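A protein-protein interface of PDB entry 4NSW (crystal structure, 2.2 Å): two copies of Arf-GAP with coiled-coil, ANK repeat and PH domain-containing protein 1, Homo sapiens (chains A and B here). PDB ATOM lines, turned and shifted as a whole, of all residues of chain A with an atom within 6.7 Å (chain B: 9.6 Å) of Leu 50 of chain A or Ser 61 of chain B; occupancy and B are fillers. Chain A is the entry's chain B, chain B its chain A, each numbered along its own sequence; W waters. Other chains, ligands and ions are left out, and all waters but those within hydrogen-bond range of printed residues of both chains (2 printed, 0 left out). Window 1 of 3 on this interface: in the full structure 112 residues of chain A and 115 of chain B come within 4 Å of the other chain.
O of Gly 49 of chain A is in hydrogen-bond range of OG of Ser 53 of chain A.
The backbone carbonyl oxygen (O) of Leu 50 of chain A is in hydrogen-bond range of the side-chain hydroxyl (OG) of Ser 53 of chain A (3.4 Å).
OG of Ser 61 of chain B lies within hydrogen-bond range of O of Tyr 57 of chain B (2.8 Å).
Ala 63 of chain B touches Leu 46 of chain A (O to CD2, 3.5 Å).
CD1 of Phe 64 of chain B touches O of Leu 46 of chain A, 3.999 Å away.
CE1 of Phe 64 of chain B touches CA of Gly 47 of chain A, 3.9 Å away.
Tyr 57 of chain B touches Leu 50 of chain A.
Ser 61 of chain B touches Leu 50 of chain A (OG to CD1, 3.7 Å).
Phe 64 of chain B touches Leu 50 of chain A (CD2 to CD1, 3.4 Å).
Ser 53 of chain A touches His 56 of chain B.
Ser 53 of chain A touches Ala 60 of chain B.
Tyr 57 of chain B touches Gly 54 of chain A (CD1 to CA, 3.3 Å).
Leu 103 of chain A touches Tyr 57 of chain B (CD2 to OH, 3.6 Å).
Of chain B, only Phe 64 (3.9 Å) comes within 4 Å of Gly 47 of chain A.
Gly 49 of chain A touches just one residue of chain B: Ala 60 (3.9 Å).
Of chain B, only Tyr 57 (3.6 Å), Ser 61 (3.7 Å) and Phe 64 (3.4 Å) come within 4 Å of Leu 50 of chain A.
Ser 61 of chain B touches just one residue of chain A: Leu 50.
Printed residues of chain A within 4 Å of Phe 64 of chain B: Leu 46 (3.999 Å), Gly 47 (3.9 Å) and Leu 50 (3.4 Å).
Printed residues of chain A within 4 Å of Gly 67 of chain B: Leu 46 (3.9 Å).
Hydrophobic or aromatic side chains of chain B within 4 Å of the printed part of chain A: His 56, Tyr 57, Ala 60 and Phe 64.
Of the 13 printed residues of chain A, 7 touch a printed residue of chain B.
Hydrophobic or aromatic side chains of chain A that line the printed part of chain B: Leu 46, Leu 50 and Leu 103.
Among the printed residues, 13 pairs touch across the chains.
Among the printed residues, no Asp or Glu carboxylate lies within 4 Å of a Lys or Arg side-chain nitrogen of the other chain.
3 positions are printed for both chains.
Of the 13 pairs that touch across the chains among the printed residues, none has its exchanged pair printed and touching as well.
Water W2 bridges the backbone carbonyl oxygen (O) of Leu 46 of chain A and the backbone carbonyl oxygen (O) of Ala 60 of chain B.
Water W1 lies within hydrogen-bond range of O of Ser 53 of chain A (2.7 Å) and O of Ser 53 of chain B (2.7 Å).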
ATOM      1  N   LYS A  45       7.925  -6.123  11.119  1.00  0.00           N
ATOM      2  CA  LYS A  45       6.932  -5.179  11.619  1.00  0.00           C
ATOM      3  C   LYS A  45       5.640  -5.889  12.172  1.00  0.00           C
ATOM      4  O   LYS A  45       5.188  -5.617  13.324  1.00  0.00           O
ATOM      5  CB  LYS A  45       6.641  -4.158  10.511  1.00  0.00           C
ATOM      6  CG  LYS A  45       6.116  -2.846  11.002  1.00  0.00           C
ATOM      7  CD  LYS A  45       5.409  -2.057   9.904  1.00  0.00           C
ATOM      8  CE  LYS A  45       4.103  -1.483  10.436  1.00  0.00           C
ATOM      9  NZ  LYS A  45       3.244  -0.997   9.314  1.00  0.00           N
ATOM     10  N   LEU A  46       5.079  -6.808  11.380  1.00  0.00           N
ATOM     11  CA  LEU A  46       3.964  -7.640  11.797  1.00  0.00           C
ATOM     12  C   LEU A  46       4.336  -8.593  12.960  1.00  0.00           C
ATOM     13  O   LEU A  46       3.468  -9.041  13.715  1.00  0.00           O
ATOM     14  CB  LEU A  46       3.510  -8.495  10.618  1.00  0.00           C
ATOM     15  CG  LEU A  46       2.272  -8.302   9.726  1.00  0.00           C
ATOM     16  CD1 LEU A  46       1.563  -6.950   9.818  1.00  0.00           C
ATOM     17  CD2 LEU A  46       2.671  -8.611   8.281  1.00  0.00           C
ATOM     18  N   GLY A  47       5.619  -8.913  13.073  1.00  0.00           N
ATOM     19  CA  GLY A  47       6.105  -9.774  14.128  1.00  0.00           C
ATOM     20  C   GLY A  47       6.137  -8.999  15.437  1.00  0.00           C
ATOM     21  O   GLY A  47       5.817  -9.539  16.486  1.00  0.00           O
ATOM     22  N   THR A  48       6.516  -7.725  15.357  1.00  0.00           N
ATOM     23  CA  THR A  48       6.417  -6.822  16.498  1.00  0.00           C
ATOM     24  C   THR A  48       4.937  -6.676  16.931  1.00  0.00           C
ATOM     25  O   THR A  48       4.624  -6.869  18.103  1.00  0.00           O
ATOM     26  CB  THR A  48       7.064  -5.459  16.190  1.00  0.00           C
ATOM     27  OG1 THR A  48       8.455  -5.655  15.886  1.00  0.00           O
ATOM     28  CG2 THR A  48       6.937  -4.539  17.379  1.00  0.00           C
ATOM     29  N   GLY A  49       4.042  -6.350  15.983  1.00  0.00           N
ATOM     30  CA  GLY A  49       2.601  -6.347  16.224  1.00  0.00           C
ATOM     31  C   GLY A  49       2.101  -7.584  16.984  1.00  0.00           C
ATOM     32  O   GLY A  49       1.383  -7.450  17.967  1.00  0.00           O
ATOM     33  N   LEU A  50       2.494  -8.784  16.538  1.00  0.00           N
ATOM     34  CA  LEU A  50       2.014 -10.032  17.112  1.00  0.00           C
ATOM     35  C   LEU A  50       2.503 -10.172  18.575  1.00  0.00           C
ATOM     36  O   LEU A  50       1.737 -10.599  19.466  1.00  0.00           O
ATOM     37  CB  LEU A  50       2.452 -11.241  16.258  1.00  0.00           C
ATOM     38  CG  LEU A  50       2.085 -12.674  16.721  1.00  0.00           C
ATOM     39  CD1 LEU A  50       2.015 -13.698  15.569  1.00  0.00           C
ATOM     40  CD2 LEU A  50       3.057 -13.164  17.785  1.00  0.00           C
ATOM     41  N   LEU A  51       3.779  -9.813  18.797  1.00  0.00           N
ATOM     42  CA  LEU A  51       4.425 -10.021  20.057  1.00  0.00           C
ATOM     43  C   LEU A  51       3.901  -9.013  21.042  1.00  0.00           C
ATOM     44  O   LEU A  51       3.609  -9.387  22.165  1.00  0.00           O
ATOM     45  CB  LEU A  51       5.951  -9.855  19.943  1.00  0.00           C
ATOM     46  CG  LEU A  51       6.960 -10.937  19.567  1.00  0.00           C
ATOM     47  CD1 LEU A  51       6.404 -11.985  18.745  1.00  0.00           C
ATOM     48  CD2 LEU A  51       8.203 -10.313  18.853  1.00  0.00           C
ATOM     49  N   GLU A  52       3.820  -7.737  20.654  1.00  0.00           N
ATOM     50  CA  GLU A  52       3.332  -6.705  21.583  1.00  0.00           C
ATOM     51  C   GLU A  52       1.863  -6.974  21.966  1.00  0.00           C
ATOM     52  O   GLU A  52       1.455  -6.754  23.115  1.00  0.00           O
ATOM     53  CB  GLU A  52       3.476  -5.273  21.020  1.00  0.00           C
ATOM     54  CG  GLU A  52       4.927  -4.708  21.108  1.00  0.00           C
ATOM     55  CD  GLU A  52       5.136  -3.377  20.318  1.00  0.00           C
ATOM     56  OE1 GLU A  52       4.191  -2.939  19.595  1.00  0.00           O
ATOM     57  OE2 GLU A  52       6.248  -2.781  20.418  1.00  0.00           O
ATOM     58  N   SER A  53       1.063  -7.434  21.019  1.00  0.00           N
ATOM     59  CA  SER A  53      -0.323  -7.678  21.378  1.00  0.00           C
ATOM     60  C   SER A  53      -0.472  -9.003  22.113  1.00  0.00           C
ATOM     61  O   SER A  53      -1.335  -9.123  22.949  1.00  0.00           O
ATOM     62  CB  SER A  53      -1.257  -7.581  20.188  1.00  0.00           C
ATOM     63  OG  SER A  53      -0.994  -8.642  19.315  1.00  0.00           O
ATOM     64  N   GLY A  54       0.377  -9.974  21.830  1.00  0.00           N
ATOM     65  CA  GLY A  54       0.415 -11.228  22.586  1.00  0.00           C
ATOM     66  C   GLY A  54       0.686 -11.006  24.072  1.00  0.00           C
ATOM     67  O   GLY A  54      -0.028 -11.536  24.900  1.00  0.00           O
ATOM     68  N   ARG A  55       1.728 -10.240  24.396  1.00  0.00           N
ATOM     69  CA  ARG A  55       2.120  -9.951  25.770  1.00  0.00           C
ATOM     70  C   ARG A  55       1.014  -9.181  26.511  1.00  0.00           C
ATOM     71  O   ARG A  55       0.795  -9.398  27.698  1.00  0.00           O
ATOM     72  CB  ARG A  55       3.426  -9.115  25.844  1.00  0.00           C
ATOM     73  CG  ARG A  55       4.625  -9.648  25.073  1.00  0.00           C
ATOM     74  CD  ARG A  55       5.355 -10.816  25.774  1.00  0.00           C
ATOM     75  NE  ARG A  55       6.414 -11.352  24.907  1.00  0.00           N
ATOM     76  CZ  ARG A  55       6.951 -12.579  25.003  1.00  0.00           C
ATOM     77  NH1 ARG A  55       6.541 -13.443  25.950  1.00  0.00           N
ATOM     78  NH2 ARG A  55       7.929 -12.945  24.145  1.00  0.00           N
ATOM     79  N   LEU A 103       5.561 -17.292  22.589  1.00  0.00           N
ATOM     80  CA  LEU A 103       5.868 -15.950  22.010  1.00  0.00           C
ATOM     81  C   LEU A 103       7.390 -15.701  21.993  1.00  0.00           C
ATOM     82  O   LEU A 103       7.919 -15.128  21.053  1.00  0.00           O
ATOM     83  CB  LEU A 103       5.179 -14.834  22.788  1.00  0.00           C
ATOM     84  CG  LEU A 103       3.635 -14.801  22.720  1.00  0.00           C
ATOM     85  CD1 LEU A 103       3.107 -13.705  23.658  1.00  0.00           C
ATOM     86  CD2 LEU A 103       3.158 -14.554  21.342  1.00  0.00           C
ATOM     87  N   THR A 106       8.695 -17.690  19.057  1.00  0.00           N
ATOM     88  CA  THR A 106       8.307 -16.926  17.897  1.00  0.00           C
ATOM     89  C   THR A 106       9.246 -15.750  17.676  1.00  0.00           C
ATOM     90  O   THR A 106       9.694 -15.504  16.533  1.00  0.00           O
ATOM     91  CB  THR A 106       6.821 -16.452  17.998  1.00  0.00           C
ATOM     92  OG1 THR A 106       5.977 -17.589  18.133  1.00  0.00           O
ATOM     93  CG2 THR A 106       6.394 -15.712  16.797  1.00  0.00           C
ATOM     94  N   SER B  53      -8.462  -7.825  24.223  1.00  0.00           N
ATOM     95  CA  SER B  53      -7.020  -8.050  24.060  1.00  0.00           C
ATOM     96  C   SER B  53      -6.739  -9.269  23.248  1.00  0.00           C
ATOM     97  O   SER B  53      -5.868  -9.244  22.417  1.00  0.00           O
ATOM     98  CB  SER B  53      -6.343  -8.246  25.430  1.00  0.00           C
ATOM     99  OG  SER B  53      -5.762  -7.013  25.785  1.00  0.00           O
ATOM    100  N   GLY B  54      -7.487 -10.324  23.520  1.00  0.00           N
ATOM    101  CA  GLY B  54      -7.417 -11.585  22.795  1.00  0.00           C
ATOM    102  C   GLY B  54      -7.743 -11.423  21.311  1.00  0.00           C
ATOM    103  O   GLY B  54      -7.035 -11.944  20.420  1.00  0.00           O
ATOM    104  N   ARG B  55      -8.811 -10.697  21.039  1.00  0.00           N
ATOM    105  CA  ARG B  55      -9.215 -10.473  19.655  1.00  0.00           C
ATOM    106  C   ARG B  55      -8.176  -9.682  18.886  1.00  0.00           C
ATOM    107  O   ARG B  55      -7.931  -9.974  17.727  1.00  0.00           O
ATOM    108  CB  ARG B  55     -10.534  -9.722  19.573  1.00  0.00           C
ATOM    109  CG  ARG B  55     -11.650 -10.391  20.263  1.00  0.00           C
ATOM    110  CD  ARG B  55     -11.839 -11.776  19.743  1.00  0.00           C
ATOM    111  NE  ARG B  55     -13.171 -12.263  20.076  1.00  0.00           N
ATOM    112  CZ  ARG B  55     -13.611 -13.480  19.783  1.00  0.00           C
ATOM    113  NH1 ARG B  55     -14.840 -13.819  20.121  1.00  0.00           N
ATOM    114  NH2 ARG B  55     -12.825 -14.357  19.178  1.00  0.00           N
ATOM    115  N   HIS B  56      -7.630  -8.644  19.505  1.00  0.00           N
ATOM    116  CA  HIS B  56      -6.645  -7.807  18.851  1.00  0.00           C
ATOM    117  C   HIS B  56      -5.387  -8.680  18.619  1.00  0.00           C
ATOM    118  O   HIS B  56      -4.717  -8.525  17.611  1.00  0.00           O
ATOM    119  CB  HIS B  56      -6.403  -6.538  19.680  1.00  0.00           C
ATOM    120  CG  HIS B  56      -5.340  -5.627  19.148  1.00  0.00           C
ATOM    121  ND1 HIS B  56      -5.602  -4.617  18.245  1.00  0.00           N
ATOM    122  CD2 HIS B  56      -4.021  -5.532  19.442  1.00  0.00           C
ATOM    123  CE1 HIS B  56      -4.485  -3.966  17.971  1.00  0.00           C
ATOM    124  NE2 HIS B  56      -3.509  -4.505  18.681  1.00  0.00           N
ATOM    125  N   TYR B  57      -5.129  -9.650  19.502  1.00  0.00           N
ATOM    126  CA  TYR B  57      -3.946 -10.512  19.342  1.00  0.00           C
ATOM    127  C   TYR B  57      -4.111 -11.550  18.241  1.00  0.00           C
ATOM    128  O   TYR B  57      -3.198 -11.779  17.467  1.00  0.00           O
ATOM    129  CB  TYR B  57      -3.565 -11.196  20.652  1.00  0.00           C
ATOM    130  CG  TYR B  57      -2.661 -12.385  20.527  1.00  0.00           C
ATOM    131  CD1 TYR B  57      -1.349 -12.265  20.021  1.00  0.00           C
ATOM    132  CD2 TYR B  57      -3.086 -13.635  20.944  1.00  0.00           C
ATOM    133  CE1 TYR B  57      -0.497 -13.372  19.965  1.00  0.00           C
ATOM    134  CE2 TYR B  57      -2.229 -14.751  20.894  1.00  0.00           C
ATOM    135  CZ  TYR B  57      -0.946 -14.599  20.404  1.00  0.00           C
ATOM    136  OH  TYR B  57      -0.123 -15.694  20.338  1.00  0.00           O
ATOM    137  N   LEU B  58      -5.281 -12.162  18.171  1.00  0.00           N
ATOM    138  CA  LEU B  58      -5.626 -13.033  17.066  1.00  0.00           C
ATOM    139  C   LEU B  58      -5.557 -12.287  15.742  1.00  0.00           C
ATOM    140  O   LEU B  58      -5.007 -12.797  14.780  1.00  0.00           O
ATOM    141  CB  LEU B  58      -7.034 -13.640  17.295  1.00  0.00           C
ATOM    142  CG  LEU B  58      -6.975 -14.538  18.530  1.00  0.00           C
ATOM    143  CD1 LEU B  58      -8.223 -15.341  18.698  1.00  0.00           C
ATOM    144  CD2 LEU B  58      -5.715 -15.445  18.495  1.00  0.00           C
ATOM    145  N   ALA B  59      -6.069 -11.056  15.702  1.00  0.00           N
ATOM    146  CA  ALA B  59      -6.075 -10.300  14.457  1.00  0.00           C
ATOM    147  C   ALA B  59      -4.642  -9.994  14.008  1.00  0.00           C
ATOM    148  O   ALA B  59      -4.332 -10.188  12.821  1.00  0.00           O
ATOM    149  CB  ALA B  59      -6.885  -9.036  14.582  1.00  0.00           C
ATOM    150  N   ALA B  60      -3.780  -9.552  14.938  1.00  0.00           N
ATOM    151  CA  ALA B  60      -2.346  -9.331  14.622  1.00  0.00           C
ATOM    152  C   ALA B  60      -1.665 -10.614  14.171  1.00  0.00           C
ATOM    153  O   ALA B  60      -0.811 -10.573  13.317  1.00  0.00           O
ATOM    154  CB  ALA B  60      -1.557  -8.690  15.776  1.00  0.00           C
ATOM    155  N   SER B  61      -2.054 -11.737  14.753  1.00  0.00           N
ATOM    156  CA  SER B  61      -1.519 -13.036  14.361  1.00  0.00           C
ATOM    157  C   SER B  61      -1.924 -13.463  12.964  1.00  0.00           C
ATOM    158  O   SER B  61      -1.062 -13.993  12.229  1.00  0.00           O
ATOM    159  CB  SER B  61      -1.950 -14.123  15.320  1.00  0.00           C
ATOM    160  OG  SER B  61      -1.535 -13.803  16.610  1.00  0.00           O
ATOM    161  N   ARG B  62      -3.213 -13.256  12.615  1.00  0.00           N
ATOM    162  CA  ARG B  62      -3.687 -13.586  11.281  1.00  0.00           C
ATOM    163  C   ARG B  62      -2.906 -12.791  10.265  1.00  0.00           C
ATOM    164  O   ARG B  62      -2.542 -13.313   9.209  1.00  0.00           O
ATOM    165  CB  ARG B  62      -5.193 -13.283  11.063  1.00  0.00           C
ATOM    166  CG  ARG B  62      -6.139 -14.139  11.873  1.00  0.00           C
ATOM    167  CD  ARG B  62      -7.662 -13.908  11.559  1.00  0.00           C
ATOM    168  NE  ARG B  62      -8.402 -14.514  12.672  1.00  0.00           N
ATOM    169  CZ  ARG B  62      -8.965 -13.848  13.694  1.00  0.00           C
ATOM    170  NH1 ARG B  62      -8.987 -12.510  13.737  1.00  0.00           N
ATOM    171  NH2 ARG B  62      -9.557 -14.537  14.666  1.00  0.00           N
ATOM    172  N   ALA B  63      -2.668 -11.517  10.564  1.00  0.00           N
ATOM    173  CA  ALA B  63      -1.968 -10.642   9.633  1.00  0.00           C
ATOM    174  C   ALA B  63      -0.495 -11.055   9.524  1.00  0.00           C
ATOM    175  O   ALA B  63       0.105 -10.921   8.469  1.00  0.00           O
ATOM    176  CB  ALA B  63      -2.099  -9.210  10.067  1.00  0.00           C
ATOM    177  N   PHE B  64       0.079 -11.557  10.617  1.00  0.00           N
ATOM    178  CA  PHE B  64       1.443 -12.129  10.586  1.00  0.00           C
ATOM    179  C   PHE B  64       1.508 -13.299   9.597  1.00  0.00           C
ATOM    180  O   PHE B  64       2.414 -13.384   8.773  1.00  0.00           O
ATOM    181  CB  PHE B  64       1.824 -12.609  11.977  1.00  0.00           C
ATOM    182  CG  PHE B  64       3.196 -13.233  12.098  1.00  0.00           C
ATOM    183  CD1 PHE B  64       4.329 -12.500  11.902  1.00  0.00           C
ATOM    184  CD2 PHE B  64       3.330 -14.555  12.529  1.00  0.00           C
ATOM    185  CE1 PHE B  64       5.590 -13.089  12.076  1.00  0.00           C
ATOM    186  CE2 PHE B  64       4.587 -15.131  12.754  1.00  0.00           C
ATOM    187  CZ  PHE B  64       5.715 -14.403  12.506  1.00  0.00           C
ATOM    188  N   VAL B  65       0.528 -14.192   9.688  1.00  0.00           N
ATOM    189  CA  VAL B  65       0.453 -15.321   8.770  1.00  0.00           C
ATOM    190  C   VAL B  65       0.222 -14.876   7.329  1.00  0.00           C
ATOM    191  O   VAL B  65       0.898 -15.353   6.411  1.00  0.00           O
ATOM    192  CB  VAL B  65      -0.565 -16.365   9.249  1.00  0.00           C
ATOM    193  CG1 VAL B  65      -0.607 -17.572   8.271  1.00  0.00           C
ATOM    194  CG2 VAL B  65      -0.175 -16.801  10.650  1.00  0.00           C
ATOM    195  N   VAL B  66      -0.644 -13.897   7.120  1.00  0.00           N
ATOM    196  CA  VAL B  66      -0.753 -13.312   5.755  1.00  0.00           C
ATOM    197  C   VAL B  66       0.623 -12.799   5.271  1.00  0.00           C
ATOM    198  O   VAL B  66       0.998 -13.017   4.123  1.00  0.00           O
ATOM    199  CB  VAL B  66      -1.871 -12.246   5.631  1.00  0.00           C
ATOM    200  CG1 VAL B  66      -1.906 -11.631   4.223  1.00  0.00           C
ATOM    201  CG2 VAL B  66      -3.204 -12.884   5.940  1.00  0.00           C
ATOM    202  N   GLY B  67       1.398 -12.190   6.176  1.00  0.00           N
ATOM    203  CA  GLY B  67       2.716 -11.660   5.839  1.00  0.00           C
ATOM    204  C   GLY B  67       3.715 -12.724   5.452  1.00  0.00           C
ATOM    205  O   GLY B  67       4.580 -12.494   4.600  1.00  0.00           O
ATOM    206  N   ILE B  68       3.592 -13.891   6.073  1.00  0.00           N
ATOM    207  CA  ILE B  68       4.475 -15.008   5.799  1.00  0.00           C
ATOM    208  C   ILE B  68       4.318 -15.479   4.333  1.00  0.00           C
ATOM    209  O   ILE B  68       5.307 -15.637   3.621  1.00  0.00           O
ATOM    210  CB  ILE B  68       4.245 -16.192   6.794  1.00  0.00           C
ATOM    211  CG1 ILE B  68       4.684 -15.824   8.217  1.00  0.00           C
ATOM    212  CG2 ILE B  68       5.037 -17.401   6.353  1.00  0.00           C
ATOM    213  CD1 ILE B  68       4.223 -16.820   9.295  1.00  0.00           C
ATOM    214  N   CYS B  69       3.080 -15.690   3.896  1.00  0.00           N
ATOM    215  CA  CYS B  69       2.771 -16.036   2.506  1.00  0.00           C
ATOM    216  C   CYS B  69       3.277 -15.019   1.492  1.00  0.00           C
ATOM    217  O   CYS B  69       4.038 -15.358   0.572  1.00  0.00           O
ATOM    218  CB  CYS B  69       1.281 -16.209   2.351  1.00  0.00           C
ATOM    219  SG  CYS B  69       0.692 -17.366   3.541  1.00  0.00           S
ATOM    220  N   THR B  89       0.751 -22.703   6.861  1.00  0.00           N
ATOM    221  CA  THR B  89      -0.092 -21.526   7.054  1.00  0.00           C
ATOM    222  C   THR B  89      -1.524 -21.929   7.390  1.00  0.00           C
ATOM    223  O   THR B  89      -2.215 -21.205   8.105  1.00  0.00           O
ATOM    224  CB  THR B  89      -0.121 -20.544   5.860  1.00  0.00           C
ATOM    225  OG1 THR B  89      -0.738 -21.164   4.743  1.00  0.00           O
ATOM    226  CG2 THR B  89       1.258 -20.082   5.487  1.00  0.00           C
ATOM    227  N   LEU B  92      -1.290 -22.974  11.196  1.00  0.00           N
ATOM    228  CA  LEU B  92      -1.184 -21.809  12.045  1.00  0.00           C
ATOM    229  C   LEU B  92      -2.528 -21.084  12.092  1.00  0.00           C
ATOM    230  O   LEU B  92      -2.952 -20.664  13.151  1.00  0.00           O
ATOM    231  CB  LEU B  92      -0.045 -20.866  11.594  1.00  0.00           C
ATOM    232  CG  LEU B  92       1.448 -21.271  11.755  1.00  0.00           C
ATOM    233  CD1 LEU B  92       2.383 -20.446  10.869  1.00  0.00           C
ATOM    234  CD2 LEU B  92       1.964 -21.226  13.180  1.00  0.00           C
ATOM    235  N   ASN B  93      -3.183 -20.928  10.948  1.00  0.00           N
ATOM    236  CA  ASN B  93      -4.509 -20.352  10.922  1.00  0.00           C
ATOM    237  C   ASN B  93      -5.486 -21.157  11.716  1.00  0.00           C
ATOM    238  O   ASN B  93      -6.385 -20.594  12.319  1.00  0.00           O
ATOM    239  CB  ASN B  93      -5.043 -20.177   9.513  1.00  0.00           C
ATOM    240  CG  ASN B  93      -4.610 -18.885   8.913  1.00  0.00           C
ATOM    241  OD1 ASN B  93      -4.364 -17.913   9.639  1.00  0.00           O
ATOM    242  ND2 ASN B  93      -4.476 -18.855   7.583  1.00  0.00           N
ATOM    243  N   HIS B  94      -5.317 -22.476  11.707  1.00  0.00           N
ATOM    244  CA  HIS B  94      -6.185 -23.355  12.484  1.00  0.00           C
ATOM    245  C   HIS B  94      -6.136 -23.030  13.983  1.00  0.00           C
ATOM    246  O   HIS B  94      -7.189 -22.920  14.640  1.00  0.00           O
ATOM    247  CB  HIS B  94      -5.825 -24.816  12.220  1.00  0.00           C
ATOM    248  CG  HIS B  94      -6.597 -25.781  13.062  1.00  0.00           C
ATOM    249  ND1 HIS B  94      -6.062 -26.377  14.185  1.00  0.00           N
ATOM    250  CD2 HIS B  94      -7.877 -26.226  12.962  1.00  0.00           C
ATOM    251  CE1 HIS B  94      -6.982 -27.151  14.737  1.00  0.00           C
ATOM    252  NE2 HIS B  94      -8.089 -27.080  14.010  1.00  0.00           N
ATOM    253  N   LYS B  95      -4.921 -22.838  14.504  1.00  0.00           N
ATOM    254  CA  LYS B  95      -4.691 -22.565  15.925  1.00  0.00           C
ATOM    255  C   LYS B  95      -5.384 -21.274  16.359  1.00  0.00           C
ATOM    256  O   LYS B  95      -5.912 -21.190  17.459  1.00  0.00           O
ATOM    257  CB  LYS B  95      -3.177 -22.474  16.253  1.00  0.00           C
ATOM    258  CG  LYS B  95      -2.382 -23.756  16.022  1.00  0.00           C
ATOM    259  CD  LYS B  95      -3.155 -25.019  16.373  1.00  0.00           C
ATOM    260  CE  LYS B  95      -2.590 -26.267  15.632  1.00  0.00           C
ATOM    261  NZ  LYS B  95      -2.853 -26.290  14.163  1.00  0.00           N
ATOM    262  N   LEU B  96      -5.394 -20.287  15.472  1.00  0.00           N
ATOM    263  CA  LEU B  96      -6.104 -19.016  15.670  1.00  0.00           C
ATOM    264  C   LEU B  96      -7.596 -19.190  15.678  1.00  0.00           C
ATOM    265  O   LEU B  96      -8.265 -18.487  16.421  1.00  0.00           O
ATOM    266  CB  LEU B  96      -5.707 -17.988  14.600  1.00  0.00           C
ATOM    267  CG  LEU B  96      -4.182 -17.821  14.496  1.00  0.00           C
ATOM    268  CD1 LEU B  96      -3.814 -16.887  13.373  1.00  0.00           C
ATOM    269  CD2 LEU B  96      -3.484 -17.410  15.849  1.00  0.00           C
ATOM    270  N   ASP B  97      -8.122 -20.095  14.850  1.00  0.00           N
ATOM    271  CA  ASP B  97      -9.569 -20.371  14.834  1.00  0.00           C
ATOM    272  C   ASP B  97     -10.007 -21.056  16.127  1.00  0.00           C
ATOM    273  O   ASP B  97     -10.991 -20.689  16.722  1.00  0.00           O
ATOM    274  CB  ASP B  97      -9.980 -21.207  13.617  1.00  0.00           C
ATOM    275  CG  ASP B  97      -9.928 -20.419  12.336  1.00  0.00           C
ATOM    276  OD1 ASP B  97      -9.685 -19.195  12.413  1.00  0.00           O
ATOM    277  OD2 ASP B  97     -10.106 -21.014  11.248  1.00  0.00           O
ATOM    278  N   HIS B  99      -8.516 -20.814  18.813  1.00  0.00           N
ATOM    279  CA  HIS B  99      -8.293 -19.900  19.887  1.00  0.00           C
ATOM    280  C   HIS B  99      -9.443 -18.941  19.967  1.00  0.00           C
ATOM    281  O   HIS B  99      -9.883 -18.610  21.071  1.00  0.00           O
ATOM    282  CB  HIS B  99      -6.973 -19.153  19.738  1.00  0.00           C
ATOM    283  CG  HIS B  99      -6.531 -18.488  20.994  1.00  0.00           C
ATOM    284  ND1 HIS B  99      -5.236 -18.556  21.460  1.00  0.00           N
ATOM    285  CD2 HIS B  99      -7.216 -17.741  21.895  1.00  0.00           C
ATOM    286  CE1 HIS B  99      -5.152 -17.900  22.604  1.00  0.00           C
ATOM    287  NE2 HIS B  99      -6.339 -17.395  22.884  1.00  0.00           N
HETATM  288  O   HOH W   1      -3.619  -7.677  22.580  1.00  0.00           O
HETATM  289  O   HOH W   2       1.037  -8.727  13.274  1.00  0.00           O
